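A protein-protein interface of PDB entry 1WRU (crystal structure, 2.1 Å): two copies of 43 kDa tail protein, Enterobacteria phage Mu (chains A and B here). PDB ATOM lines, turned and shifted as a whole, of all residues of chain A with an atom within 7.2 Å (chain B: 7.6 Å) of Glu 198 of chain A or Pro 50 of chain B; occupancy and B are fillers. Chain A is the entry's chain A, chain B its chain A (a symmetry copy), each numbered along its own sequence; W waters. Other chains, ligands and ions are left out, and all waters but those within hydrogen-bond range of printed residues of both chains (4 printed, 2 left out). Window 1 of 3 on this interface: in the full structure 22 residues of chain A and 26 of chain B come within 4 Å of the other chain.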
ATOM      1  N   PHE A 196      17.952  -7.163 -19.778  1.00  0.00           N
ATOM      2  CA  PHE A 196      17.093  -6.001 -19.957  1.00  0.00           C
ATOM      3  C   PHE A 196      17.134  -5.567 -21.428  1.00  0.00           C
ATOM      4  O   PHE A 196      18.203  -5.239 -21.982  1.00  0.00           O
ATOM      5  CB  PHE A 196      17.577  -4.874 -19.047  1.00  0.00           C
ATOM      6  CG  PHE A 196      16.784  -3.600 -19.167  1.00  0.00           C
ATOM      7  CD1 PHE A 196      15.442  -3.620 -19.514  1.00  0.00           C
ATOM      8  CD2 PHE A 196      17.383  -2.374 -18.920  1.00  0.00           C
ATOM      9  CE1 PHE A 196      14.718  -2.437 -19.619  1.00  0.00           C
ATOM     10  CE2 PHE A 196      16.660  -1.189 -19.020  1.00  0.00           C
ATOM     11  CZ  PHE A 196      15.331  -1.222 -19.372  1.00  0.00           C
ATOM     12  N   GLU A 197      15.957  -5.570 -22.038  1.00  0.00           N
ATOM     13  CA  GLU A 197      15.801  -5.224 -23.446  1.00  0.00           C
ATOM     14  C   GLU A 197      14.848  -4.047 -23.671  1.00  0.00           C
ATOM     15  O   GLU A 197      13.683  -4.076 -23.243  1.00  0.00           O
ATOM     16  CB  GLU A 197      15.282  -6.442 -24.196  1.00  0.00           C
ATOM     17  CG  GLU A 197      14.910  -6.179 -25.628  1.00  0.00           C
ATOM     18  CD  GLU A 197      16.034  -6.515 -26.575  1.00  0.00           C
ATOM     19  OE1 GLU A 197      16.449  -7.699 -26.618  1.00  0.00           O
ATOM     20  OE2 GLU A 197      16.503  -5.594 -27.270  1.00  0.00           O
ATOM     21  N   GLU A 198      15.350  -3.013 -24.333  1.00  0.00           N
ATOM     22  CA  GLU A 198      14.544  -1.828 -24.655  1.00  0.00           C
ATOM     23  C   GLU A 198      14.473  -1.803 -26.179  1.00  0.00           C
ATOM     24  O   GLU A 198      15.439  -1.436 -26.854  1.00  0.00           O
ATOM     25  CB  GLU A 198      15.214  -0.542 -24.157  1.00  0.00           C
ATOM     26  CG  GLU A 198      15.476  -0.495 -22.657  1.00  0.00           C
ATOM     27  CD  GLU A 198      16.578   0.488 -22.313  1.00  0.00           C
ATOM     28  OE1 GLU A 198      16.310   1.709 -22.264  1.00  0.00           O
ATOM     29  OE2 GLU A 198      17.720   0.031 -22.119  1.00  0.00           O
ATOM     30  N   ASP A 199      13.325  -2.189 -26.717  1.00  0.00           N
ATOM     31  CA  ASP A 199      13.175  -2.243 -28.163  1.00  0.00           C
ATOM     32  C   ASP A 199      12.050  -1.360 -28.667  1.00  0.00           C
ATOM     33  O   ASP A 199      10.878  -1.566 -28.335  1.00  0.00           O
ATOM     34  CB  ASP A 199      12.977  -3.708 -28.552  1.00  0.00           C
ATOM     35  CG  ASP A 199      12.709  -3.902 -30.043  1.00  0.00           C
ATOM     36  OD1 ASP A 199      12.884  -2.956 -30.826  1.00  0.00           O
ATOM     37  OD2 ASP A 199      12.319  -5.022 -30.421  1.00  0.00           O
ATOM     38  N   PHE A 200      12.407  -0.363 -29.469  1.00  0.00           N
ATOM     39  CA  PHE A 200      11.427   0.567 -30.017  1.00  0.00           C
ATOM     40  C   PHE A 200      11.046   0.335 -31.479  1.00  0.00           C
ATOM     41  O   PHE A 200      10.368   1.159 -32.093  1.00  0.00           O
ATOM     42  CB  PHE A 200      11.912   2.004 -29.850  1.00  0.00           C
ATOM     43  CG  PHE A 200      11.760   2.520 -28.464  1.00  0.00           C
ATOM     44  CD1 PHE A 200      12.382   1.873 -27.399  1.00  0.00           C
ATOM     45  CD2 PHE A 200      10.947   3.614 -28.206  1.00  0.00           C
ATOM     46  CE1 PHE A 200      12.190   2.310 -26.087  1.00  0.00           C
ATOM     47  CE2 PHE A 200      10.745   4.063 -26.898  1.00  0.00           C
ATOM     48  CZ  PHE A 200      11.368   3.407 -25.835  1.00  0.00           C
ATOM     49  N   ARG A 201      11.429  -0.803 -32.033  1.00  0.00           N
ATOM     50  CA  ARG A 201      11.109  -1.033 -33.439  1.00  0.00           C
ATOM     51  C   ARG A 201       9.605  -0.989 -33.709  1.00  0.00           C
ATOM     52  O   ARG A 201       9.183  -0.490 -34.738  1.00  0.00           O
ATOM     53  CB  ARG A 201      11.709  -2.363 -33.900  1.00  0.00           C
ATOM     54  CG  ARG A 201      13.226  -2.313 -34.034  1.00  0.00           C
ATOM     55  CD  ARG A 201      13.776  -3.710 -34.282  1.00  0.00           C
ATOM     56  NE  ARG A 201      13.169  -4.639 -33.342  1.00  0.00           N
ATOM     57  CZ  ARG A 201      13.280  -5.962 -33.400  1.00  0.00           C
ATOM     58  NH1 ARG A 201      13.997  -6.537 -34.364  1.00  0.00           N
ATOM     59  NH2 ARG A 201      12.635  -6.717 -32.512  1.00  0.00           N
ATOM     60  N   ARG A 203       7.256   0.557 -31.672  1.00  0.00           N
ATOM     61  CA  ARG A 203       6.647   1.611 -30.860  1.00  0.00           C
ATOM     62  C   ARG A 203       6.360   2.776 -31.787  1.00  0.00           C
ATOM     63  O   ARG A 203       7.183   3.101 -32.644  1.00  0.00           O
ATOM     64  CB  ARG A 203       7.609   2.097 -29.765  1.00  0.00           C
ATOM     65  CG  ARG A 203       7.900   1.109 -28.644  1.00  0.00           C
ATOM     66  CD  ARG A 203       6.760   1.038 -27.627  1.00  0.00           C
ATOM     67  NE  ARG A 203       6.638   2.244 -26.806  1.00  0.00           N
ATOM     68  CZ  ARG A 203       7.395   2.526 -25.746  1.00  0.00           C
ATOM     69  NH1 ARG A 203       8.352   1.696 -25.352  1.00  0.00           N
ATOM     70  NH2 ARG A 203       7.180   3.641 -25.063  1.00  0.00           N
ATOM     71  N   ASP A 239       7.153   8.481 -25.033  1.00  0.00           N
ATOM     72  CA  ASP A 239       8.492   7.911 -25.063  1.00  0.00           C
ATOM     73  C   ASP A 239       9.087   7.900 -26.471  1.00  0.00           C
ATOM     74  O   ASP A 239      10.302   7.824 -26.631  1.00  0.00           O
ATOM     75  CB  ASP A 239       8.472   6.495 -24.475  1.00  0.00           C
ATOM     76  CG  ASP A 239       8.323   6.495 -22.956  1.00  0.00           C
ATOM     77  OD1 ASP A 239       7.896   5.464 -22.391  1.00  0.00           O
ATOM     78  OD2 ASP A 239       8.641   7.524 -22.323  1.00  0.00           O
ATOM     79  N   THR A 241      10.211   9.858 -29.267  1.00  0.00           N
ATOM     80  CA  THR A 241      10.680  11.203 -29.609  1.00  0.00           C
ATOM     81  C   THR A 241      10.412  11.752 -31.008  1.00  0.00           C
ATOM     82  O   THR A 241      10.256  12.962 -31.175  1.00  0.00           O
ATOM     83  CB  THR A 241      12.198  11.301 -29.360  1.00  0.00           C
ATOM     84  OG1 THR A 241      12.446  11.336 -27.951  1.00  0.00           O
ATOM     85  CG2 THR A 241      12.784  12.539 -30.019  1.00  0.00           C
ATOM     86  N   ARG A 242      10.375  10.889 -32.017  1.00  0.00           N
ATOM     87  CA  ARG A 242      10.144  11.362 -33.379  1.00  0.00           C
ATOM     88  C   ARG A 242       8.740  11.053 -33.890  1.00  0.00           C
ATOM     89  O   ARG A 242       8.007  10.263 -33.290  1.00  0.00           O
ATOM     90  CB  ARG A 242      11.181  10.748 -34.325  1.00  0.00           C
ATOM     91  CG  ARG A 242      10.695   9.548 -35.116  1.00  0.00           C
ATOM     92  CD  ARG A 242      11.858   8.865 -35.820  1.00  0.00           C
ATOM     93  NE  ARG A 242      12.727   8.301 -34.813  1.00  0.00           N
ATOM     94  CZ  ARG A 242      13.020   7.011 -34.704  1.00  0.00           C
ATOM     95  NH1 ARG A 242      12.533   6.119 -35.564  1.00  0.00           N
ATOM     96  NH2 ARG A 242      13.750   6.611 -33.677  1.00  0.00           N
ATOM     97  N   LYS A 273       5.753  -5.223 -24.946  1.00  0.00           N
ATOM     98  CA  LYS A 273       6.742  -5.976 -25.695  1.00  0.00           C
ATOM     99  C   LYS A 273       8.017  -5.185 -25.953  1.00  0.00           C
ATOM    100  O   LYS A 273       9.029  -5.740 -26.343  1.00  0.00           O
ATOM    101  CB  LYS A 273       6.134  -6.426 -27.030  1.00  0.00           C
ATOM    102  CG  LYS A 273       4.890  -7.299 -26.871  1.00  0.00           C
ATOM    103  CD  LYS A 273       5.195  -8.560 -26.067  1.00  0.00           C
ATOM    104  CE  LYS A 273       3.990  -9.505 -25.993  1.00  0.00           C
ATOM    105  NZ  LYS A 273       4.298 -10.772 -25.261  1.00  0.00           N
ATOM    106  N   SER A 274       7.965  -3.881 -25.730  1.00  0.00           N
ATOM    107  CA  SER A 274       9.116  -3.028 -25.957  1.00  0.00           C
ATOM    108  C   SER A 274      10.135  -2.986 -24.805  1.00  0.00           C
ATOM    109  O   SER A 274      11.342  -3.102 -25.029  1.00  0.00           O
ATOM    110  CB  SER A 274       8.624  -1.604 -26.256  1.00  0.00           C
ATOM    111  OG  SER A 274       9.620  -0.655 -25.955  1.00  0.00           O
ATOM    112  N   ILE A 275       9.651  -2.794 -23.583  1.00  0.00           N
ATOM    113  CA  ILE A 275      10.521  -2.685 -22.409  1.00  0.00           C
ATOM    114  C   ILE A 275      10.400  -3.972 -21.625  1.00  0.00           C
ATOM    115  O   ILE A 275       9.415  -4.184 -20.909  1.00  0.00           O
ATOM    116  CB  ILE A 275      10.079  -1.524 -21.514  1.00  0.00           C
ATOM    117  CG1 ILE A 275       9.937  -0.229 -22.340  1.00  0.00           C
ATOM    118  CG2 ILE A 275      11.063  -1.367 -20.337  1.00  0.00           C
ATOM    119  CD1 ILE A 275      11.223   0.245 -23.047  1.00  0.00           C
ATOM    120  N   THR A 276      11.387  -4.847 -21.756  1.00  0.00           N
ATOM    121  CA  THR A 276      11.303  -6.123 -21.046  1.00  0.00           C
ATOM    122  C   THR A 276      12.544  -6.563 -20.299  1.00  0.00           C
ATOM    123  O   THR A 276      13.681  -6.246 -20.674  1.00  0.00           O
ATOM    124  CB  THR A 276      10.926  -7.251 -22.003  1.00  0.00           C
ATOM    125  OG1 THR A 276      11.969  -7.415 -22.963  1.00  0.00           O
ATOM    126  CG2 THR A 276       9.628  -6.925 -22.730  1.00  0.00           C
ATOM    127  N   PHE A 277      12.307  -7.309 -19.225  1.00  0.00           N
ATOM    128  CA  PHE A 277      13.386  -7.845 -18.425  1.00  0.00           C
ATOM    129  C   PHE A 277      13.158  -9.342 -18.320  1.00  0.00           C
ATOM    130  O   PHE A 277      12.025  -9.802 -18.046  1.00  0.00           O
ATOM    131  CB  PHE A 277      13.381  -7.278 -16.995  1.00  0.00           C
ATOM    132  CG  PHE A 277      13.535  -5.782 -16.912  1.00  0.00           C
ATOM    133  CD1 PHE A 277      12.469  -4.942 -17.194  1.00  0.00           C
ATOM    134  CD2 PHE A 277      14.745  -5.216 -16.511  1.00  0.00           C
ATOM    135  CE1 PHE A 277      12.603  -3.557 -17.075  1.00  0.00           C
ATOM    136  CE2 PHE A 277      14.888  -3.829 -16.386  1.00  0.00           C
ATOM    137  CZ  PHE A 277      13.818  -3.005 -16.668  1.00  0.00           C
ATOM    138  N   ILE A 307      21.294   0.289 -13.035  1.00  0.00           N
ATOM    139  CA  ILE A 307      19.902  -0.071 -13.251  1.00  0.00           C
ATOM    140  C   ILE A 307      19.096  -0.276 -11.972  1.00  0.00           C
ATOM    141  O   ILE A 307      19.330  -1.217 -11.209  1.00  0.00           O
ATOM    142  CB  ILE A 307      19.786  -1.340 -14.131  1.00  0.00           C
ATOM    143  CG1 ILE A 307      20.214  -1.007 -15.564  1.00  0.00           C
ATOM    144  CG2 ILE A 307      18.345  -1.871 -14.114  1.00  0.00           C
ATOM    145  CD1 ILE A 307      20.225  -2.190 -16.504  1.00  0.00           C
ATOM    146  N   LEU B  45      25.950   4.449 -20.529  1.00  0.00           N
ATOM    147  CA  LEU B  45      25.433   4.041 -21.822  1.00  0.00           C
ATOM    148  C   LEU B  45      24.223   4.876 -22.195  1.00  0.00           C
ATOM    149  O   LEU B  45      23.436   4.495 -23.060  1.00  0.00           O
ATOM    150  CB  LEU B  45      25.051   2.569 -21.759  1.00  0.00           C
ATOM    151  CG  LEU B  45      26.119   1.777 -21.011  1.00  0.00           C
ATOM    152  CD1 LEU B  45      25.650   0.365 -20.726  1.00  0.00           C
ATOM    153  CD2 LEU B  45      27.391   1.763 -21.836  1.00  0.00           C
ATOM    154  N   SER B  46      24.085   6.022 -21.539  1.00  0.00           N
ATOM    155  CA  SER B  46      22.959   6.916 -21.774  1.00  0.00           C
ATOM    156  C   SER B  46      22.841   7.345 -23.229  1.00  0.00           C
ATOM    157  O   SER B  46      21.747   7.649 -23.706  1.00  0.00           O
ATOM    158  CB  SER B  46      23.089   8.161 -20.896  1.00  0.00           C
ATOM    159  OG  SER B  46      24.202   8.948 -21.290  1.00  0.00           O
ATOM    160  N   GLY B  47      23.968   7.369 -23.931  1.00  0.00           N
ATOM    161  CA  GLY B  47      23.960   7.780 -25.322  1.00  0.00           C
ATOM    162  C   GLY B  47      23.486   6.728 -26.311  1.00  0.00           C
ATOM    163  O   GLY B  47      23.100   7.066 -27.426  1.00  0.00           O
ATOM    164  N   LEU B  48      23.521   5.463 -25.904  1.00  0.00           N
ATOM    165  CA  LEU B  48      23.097   4.352 -26.752  1.00  0.00           C
ATOM    166  C   LEU B  48      21.619   4.005 -26.554  1.00  0.00           C
ATOM    167  O   LEU B  48      21.186   2.907 -26.882  1.00  0.00           O
ATOM    168  CB  LEU B  48      23.947   3.126 -26.434  1.00  0.00           C
ATOM    169  CG  LEU B  48      25.449   3.400 -26.456  1.00  0.00           C
ATOM    170  CD1 LEU B  48      26.198   2.189 -25.947  1.00  0.00           C
ATOM    171  CD2 LEU B  48      25.879   3.757 -27.858  1.00  0.00           C
ATOM    172  N   ALA B  49      20.854   4.953 -26.024  1.00  0.00           N
ATOM    173  CA  ALA B  49      19.431   4.744 -25.756  1.00  0.00           C
ATOM    174  C   ALA B  49      18.576   4.708 -27.022  1.00  0.00           C
ATOM    175  O   ALA B  49      18.841   5.448 -27.971  1.00  0.00           O
ATOM    176  CB  ALA B  49      18.922   5.854 -24.835  1.00  0.00           C
ATOM    177  N   PRO B  50      17.542   3.840 -27.054  1.00  0.00           N
ATOM    178  CA  PRO B  50      16.666   3.753 -28.223  1.00  0.00           C
ATOM    179  C   PRO B  50      16.170   5.159 -28.543  1.00  0.00           C
ATOM    180  O   PRO B  50      15.995   5.966 -27.637  1.00  0.00           O
ATOM    181  CB  PRO B  50      15.543   2.853 -27.735  1.00  0.00           C
ATOM    182  CG  PRO B  50      16.258   1.906 -26.847  1.00  0.00           C
ATOM    183  CD  PRO B  50      17.160   2.831 -26.050  1.00  0.00           C
ATOM    184  N   GLY B  51      15.976   5.464 -29.824  1.00  0.00           N
ATOM    185  CA  GLY B  51      15.497   6.790 -30.196  1.00  0.00           C
ATOM    186  C   GLY B  51      16.607   7.787 -30.493  1.00  0.00           C
ATOM    187  O   GLY B  51      16.392   8.779 -31.201  1.00  0.00           O
ATOM    188  N   LYS B  52      17.794   7.534 -29.947  1.00  0.00           N
ATOM    189  CA  LYS B  52      18.953   8.396 -30.159  1.00  0.00           C
ATOM    190  C   LYS B  52      19.397   8.394 -31.619  1.00  0.00           C
ATOM    191  O   LYS B  52      19.470   7.346 -32.262  1.00  0.00           O
ATOM    192  CB  LYS B  52      20.123   7.941 -29.284  1.00  0.00           C
ATOM    193  CG  LYS B  52      19.979   8.274 -27.798  1.00  0.00           C
ATOM    194  CD  LYS B  52      20.036   9.778 -27.564  1.00  0.00           C
ATOM    195  CE  LYS B  52      19.975  10.122 -26.081  1.00  0.00           C
ATOM    196  NZ  LYS B  52      20.005  11.597 -25.858  1.00  0.00           N
ATOM    197  N   LYS B  53      19.683   9.580 -32.134  1.00  0.00           N
ATOM    198  CA  LYS B  53      20.142   9.740 -33.501  1.00  0.00           C
ATOM    199  C   LYS B  53      21.571   9.214 -33.527  1.00  0.00           C
ATOM    200  O   LYS B  53      22.332   9.453 -32.594  1.00  0.00           O
ATOM    201  CB  LYS B  53      20.111  11.222 -33.862  1.00  0.00           C
ATOM    202  CG  LYS B  53      20.208  11.507 -35.335  1.00  0.00           C
ATOM    203  CD  LYS B  53      19.741  12.925 -35.627  1.00  0.00           C
ATOM    204  CE  LYS B  53      18.281  13.116 -35.225  1.00  0.00           C
ATOM    205  NZ  LYS B  53      17.745  14.452 -35.616  1.00  0.00           N
ATOM    206  N   TYR B  67      18.235   6.160 -36.523  1.00  0.00           N
ATOM    207  CA  TYR B  67      17.963   6.206 -35.102  1.00  0.00           C
ATOM    208  C   TYR B  67      18.208   4.846 -34.488  1.00  0.00           C
ATOM    209  O   TYR B  67      18.032   3.828 -35.146  1.00  0.00           O
ATOM    210  CB  TYR B  67      16.513   6.614 -34.854  1.00  0.00           C
ATOM    211  CG  TYR B  67      16.169   7.975 -35.412  1.00  0.00           C
ATOM    212  CD1 TYR B  67      15.754   8.127 -36.739  1.00  0.00           C
ATOM    213  CD2 TYR B  67      16.284   9.113 -34.625  1.00  0.00           C
ATOM    214  CE1 TYR B  67      15.462   9.388 -37.264  1.00  0.00           C
ATOM    215  CE2 TYR B  67      15.998  10.378 -35.138  1.00  0.00           C
ATOM    216  CZ  TYR B  67      15.586  10.505 -36.459  1.00  0.00           C
ATOM    217  OH  TYR B  67      15.303  11.748 -36.966  1.00  0.00           O
ATOM    218  N   ILE B  68      18.620   4.839 -33.225  1.00  0.00           N
ATOM    219  CA  ILE B  68      18.854   3.605 -32.512  1.00  0.00           C
ATOM    220  C   ILE B  68      17.479   2.963 -32.276  1.00  0.00           C
ATOM    221  O   ILE B  68      16.540   3.644 -31.874  1.00  0.00           O
ATOM    222  CB  ILE B  68      19.573   3.906 -31.175  1.00  0.00           C
ATOM    223  CG1 ILE B  68      21.043   4.268 -31.466  1.00  0.00           C
ATOM    224  CG2 ILE B  68      19.427   2.751 -30.234  1.00  0.00           C
ATOM    225  CD1 ILE B  68      21.913   4.377 -30.256  1.00  0.00           C
ATOM    226  N   ASP B  69      17.350   1.678 -32.590  1.00  0.00           N
ATOM    227  CA  ASP B  69      16.093   0.958 -32.401  1.00  0.00           C
ATOM    228  C   ASP B  69      16.042   0.248 -31.069  1.00  0.00           C
ATOM    229  O   ASP B  69      14.984   0.158 -30.422  1.00  0.00           O
ATOM    230  CB  ASP B  69      15.903  -0.142 -33.439  1.00  0.00           C
ATOM    231  CG  ASP B  69      15.440   0.373 -34.786  1.00  0.00           C
ATOM    232  OD1 ASP B  69      14.505   1.210 -34.861  1.00  0.00           O
ATOM    233  OD2 ASP B  69      16.006  -0.103 -35.782  1.00  0.00           O
ATOM    234  N   SER B  70      17.175  -0.311 -30.667  1.00  0.00           N
ATOM    235  CA  SER B  70      17.183  -1.072 -29.433  1.00  0.00           C
ATOM    236  C   SER B  70      18.477  -1.127 -28.635  1.00  0.00           C
ATOM    237  O   SER B  70      19.587  -0.965 -29.167  1.00  0.00           O
ATOM    238  CB  SER B  70      16.730  -2.496 -29.744  1.00  0.00           C
ATOM    239  OG  SER B  70      17.612  -3.109 -30.663  1.00  0.00           O
ATOM    240  N   ARG B  71      18.321  -1.347 -27.338  1.00  0.00           N
ATOM    241  CA  ARG B  71      19.460  -1.472 -26.443  1.00  0.00           C
ATOM    242  C   ARG B  71      19.194  -2.668 -25.544  1.00  0.00           C
ATOM    243  O   ARG B  71      18.095  -2.826 -24.976  1.00  0.00           O
ATOM    244  CB  ARG B  71      19.631  -0.217 -25.603  1.00  0.00           C
ATOM    245  CG  ARG B  71      20.747  -0.339 -24.581  1.00  0.00           C
ATOM    246  CD  ARG B  71      21.009   0.976 -23.880  1.00  0.00           C
ATOM    247  NE  ARG B  71      19.840   1.462 -23.149  1.00  0.00           N
ATOM    248  CZ  ARG B  71      19.772   2.649 -22.555  1.00  0.00           C
ATOM    249  NH1 ARG B  71      20.806   3.480 -22.600  1.00  0.00           N
ATOM    250  NH2 ARG B  71      18.660   3.019 -21.932  1.00  0.00           N
ATOM    251  N   ARG B  72      20.188  -3.530 -25.443  1.00  0.00           N
ATOM    252  CA  ARG B  72      20.061  -4.717 -24.621  1.00  0.00           C
ATOM    253  C   ARG B  72      21.238  -4.824 -23.667  1.00  0.00           C
ATOM    254  O   ARG B  72      22.401  -4.631 -24.057  1.00  0.00           O
ATOM    255  CB  ARG B  72      20.029  -5.962 -25.485  1.00  0.00           C
ATOM    256  CG  ARG B  72      19.677  -7.208 -24.724  1.00  0.00           C
ATOM    257  CD  ARG B  72      19.948  -8.437 -25.544  1.00  0.00           C
ATOM    258  NE  ARG B  72      19.365  -9.630 -24.942  1.00  0.00           N
ATOM    259  CZ  ARG B  72      19.349 -10.820 -25.531  1.00  0.00           C
ATOM    260  NH1 ARG B  72      19.885 -10.959 -26.735  1.00  0.00           N
ATOM    261  NH2 ARG B  72      18.792 -11.865 -24.928  1.00  0.00           N
ATOM    262  N   ARG B  73      20.927  -5.128 -22.418  1.00  0.00           N
ATOM    263  CA  ARG B  73      21.949  -5.289 -21.396  1.00  0.00           C
ATOM    264  C   ARG B  73      21.749  -6.629 -20.731  1.00  0.00           C
ATOM    265  O   ARG B  73      20.705  -6.882 -20.140  1.00  0.00           O
ATOM    266  CB  ARG B  73      21.850  -4.169 -20.371  1.00  0.00           C
ATOM    267  CG  ARG B  73      22.644  -2.940 -20.777  1.00  0.00           C
ATOM    268  CD  ARG B  73      22.324  -1.742 -19.911  1.00  0.00           C
ATOM    269  NE  ARG B  73      21.000  -1.197 -20.183  1.00  0.00           N
ATOM    270  CZ  ARG B  73      20.569  -0.021 -19.737  1.00  0.00           C
ATOM    271  NH1 ARG B  73      21.362   0.742 -18.991  1.00  0.00           N
ATOM    272  NH2 ARG B  73      19.345   0.402 -20.033  1.00  0.00           N
ATOM    273  N   THR B  83      24.274  -4.761 -26.279  1.00  0.00           N
ATOM    274  CA  THR B  83      23.984  -4.900 -27.708  1.00  0.00           C
ATOM    275  C   THR B  83      23.118  -3.720 -28.119  1.00  0.00           C
ATOM    276  O   THR B  83      22.062  -3.490 -27.542  1.00  0.00           O
ATOM    277  CB  THR B  83      23.218  -6.188 -28.002  1.00  0.00           C
ATOM    278  OG1 THR B  83      23.941  -7.298 -27.467  1.00  0.00           O
ATOM    279  CG2 THR B  83      23.039  -6.382 -29.515  1.00  0.00           C
ATOM    280  N   VAL B  84      23.568  -2.962 -29.104  1.00  0.00           N
ATOM    281  CA  VAL B  84      22.819  -1.814 -29.585  1.00  0.00           C
ATOM    282  C   VAL B  84      22.509  -2.081 -31.071  1.00  0.00           C
ATOM    283  O   VAL B  84      23.368  -2.578 -31.793  1.00  0.00           O
ATOM    284  CB  VAL B  84      23.664  -0.544 -29.426  1.00  0.00           C
ATOM    285  CG1 VAL B  84      22.866   0.679 -29.817  1.00  0.00           C
ATOM    286  CG2 VAL B  84      24.145  -0.419 -27.980  1.00  0.00           C
ATOM    287  N   ALA B  85      21.288  -1.773 -31.516  1.00  0.00           N
ATOM    288  CA  ALA B  85      20.886  -1.986 -32.912  1.00  0.00           C
ATOM    289  C   ALA B  85      20.072  -0.812 -33.460  1.00  0.00           C
ATOM    290  O   ALA B  85      19.262  -0.222 -32.743  1.00  0.00           O
ATOM    291  CB  ALA B  85      20.075  -3.286 -33.034  1.00  0.00           C
HETATM  292  O   HOH W   1      13.524   9.190 -31.708  1.00  0.00           O
HETATM  293  O   HOH W   2      13.960   4.535 -32.366  1.00  0.00           O
HETATM  294  O   HOH W   3      16.556  -3.847 -33.012  1.00  0.00           O
HETATM  295  O   HOH W   4      12.500   2.547 -33.529  1.00  0.00           O
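Of the printed residues of chain B, Glu 197 of chain A touches Ser 70, Arg 71 and Arg 72.
Of chain B, only Pro 50 (3.4 Å), Asp 69 (3.9 Å), Ser 70 (3.1 Å), Arg 71 (2.7 Å) and Arg 73 (2.7 Å) come within 4 Å of Glu 198 of chain A.
Of the printed residues of chain A, Arg 73 of chain B touches Phe 196 (2.8 Å), Glu 198 (2.7 Å) and Ile 307 (3.9 Å).
The nearest residue of chain B that does not touch Glu 198 of chain A is Arg 72 of chain B (5.0 Å).
The nearest residue of chain A that does not touch Pro 50 of chain B is Asp 199 of chain A (5.0 Å).
The nearest printed residue of chain A that does not touch Ser 70 of chain B is Phe 200 of chain A (4.8 Å).
O of Arg 71 of chain B touches O of Phe 196 of chain A (3.8 Å).
OE2 of Glu 197 of chain A touches CB of Ser 70 of chain B, at 3.97 Å.
Glu 197 of chain A touches Arg 71 of chain B (CA to O, 3.7 Å).
Asp 69 of chain B touches Glu 198 of chain A.
Ser 70 of chain B touches Glu 198 of chain A.
C of Asp 199 of chain A touches O of Asp 69 of chain B, 3.7 Å away.
Asp 199 of chain A touches Ser 70 of chain B (CA to CB, 3.9 Å).
Pro 50 of chain B touches Phe 200 of chain A.
Arg 201 of chain A touches Asp 69 of chain B (CG to CB, 3.5 Å).
CB of Tyr 67 of chain B touches NH2 of Arg 242 of chain A, 3.0 Å away.
The side-chain carboxylate (OD2) of Asp 199 of chain A is in salt-bridge range of the guanidinium group (NH2) of Arg 201 of chain A (2.7 Å).
O of Ser 274 of chain A sits at hydrogen-bond distance from N of Asp 199 of chain A (2.8 Å).
The backbone carbonyl oxygen (O) of Leu 45 of chain B lies within hydrogen-bond range of the guanidinium group (NH1) of Arg 71 of chain B (2.9 Å).
N of Asp 69 of chain B lies within hydrogen-bond range of O of Ala 85 of chain B (2.7 Å).
The backbone carbonyl oxygen of Ala 85 of chain B lies within hydrogen-bond range of the backbone NH of Ser 70 of chain B (2.9 Å).
The backbone NH (N) of Arg 72 of chain B sits at hydrogen-bond distance from the backbone carbonyl oxygen (O) of Thr 83 of chain B (2.8 Å).
No position is printed for both chains.
Water W2 lies within hydrogen-bond range of NH2 of Arg 242 of chain A (2.5 Å), O of Ile 68 of chain B (2.8 Å) and N of Gly 51 of chain B (3.4 Å).
Water W3 lies within hydrogen-bond range of OG of Ser 70 of chain B (2.7 Å) and NE of Arg 201 of chain A (3.5 Å).
Water W4 bridges the side-chain carboxylate of Asp 69 of chain B and the backbone carbonyl oxygen of Phe 200 of chain A.
Water W1 bridges O of Gly 51 of chain B and NH2 of Arg 242 of chain A.
Hydrophobic or aromatic side chains of chain A that line the printed part of chain B: Phe 196, Phe 200 and Ile 307.
Among the printed residues, Asp or Glu carboxylates within 4 Å of a Lys or Arg side-chain nitrogen of the other chain: Glu 197 of chain A with Arg 72 of chain B, Glu 198 of chain A with Arg 71 of chain B and Glu 198 of chain A with Arg 73 of chain B.
O of Phe 196 of chain A sits at hydrogen-bond distance from N of Arg 73 of chain B (2.8 Å).
The side-chain carboxylate of Glu 197 of chain A is in salt-bridge range of the guanidinium group of Arg 72 of chain B.
OE1 of Glu 198 of chain A lies within salt-bridge range of NH2 of Arg 71 of chain B, at 2.7 Å.
OE2 of Glu 198 of chain A is in salt-bridge range of NH2 of Arg 73 of chain B.
O of Asp 69 of chain B sits at hydrogen-bond distance from N of Phe 200 of chain A, at 2.8 Å.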
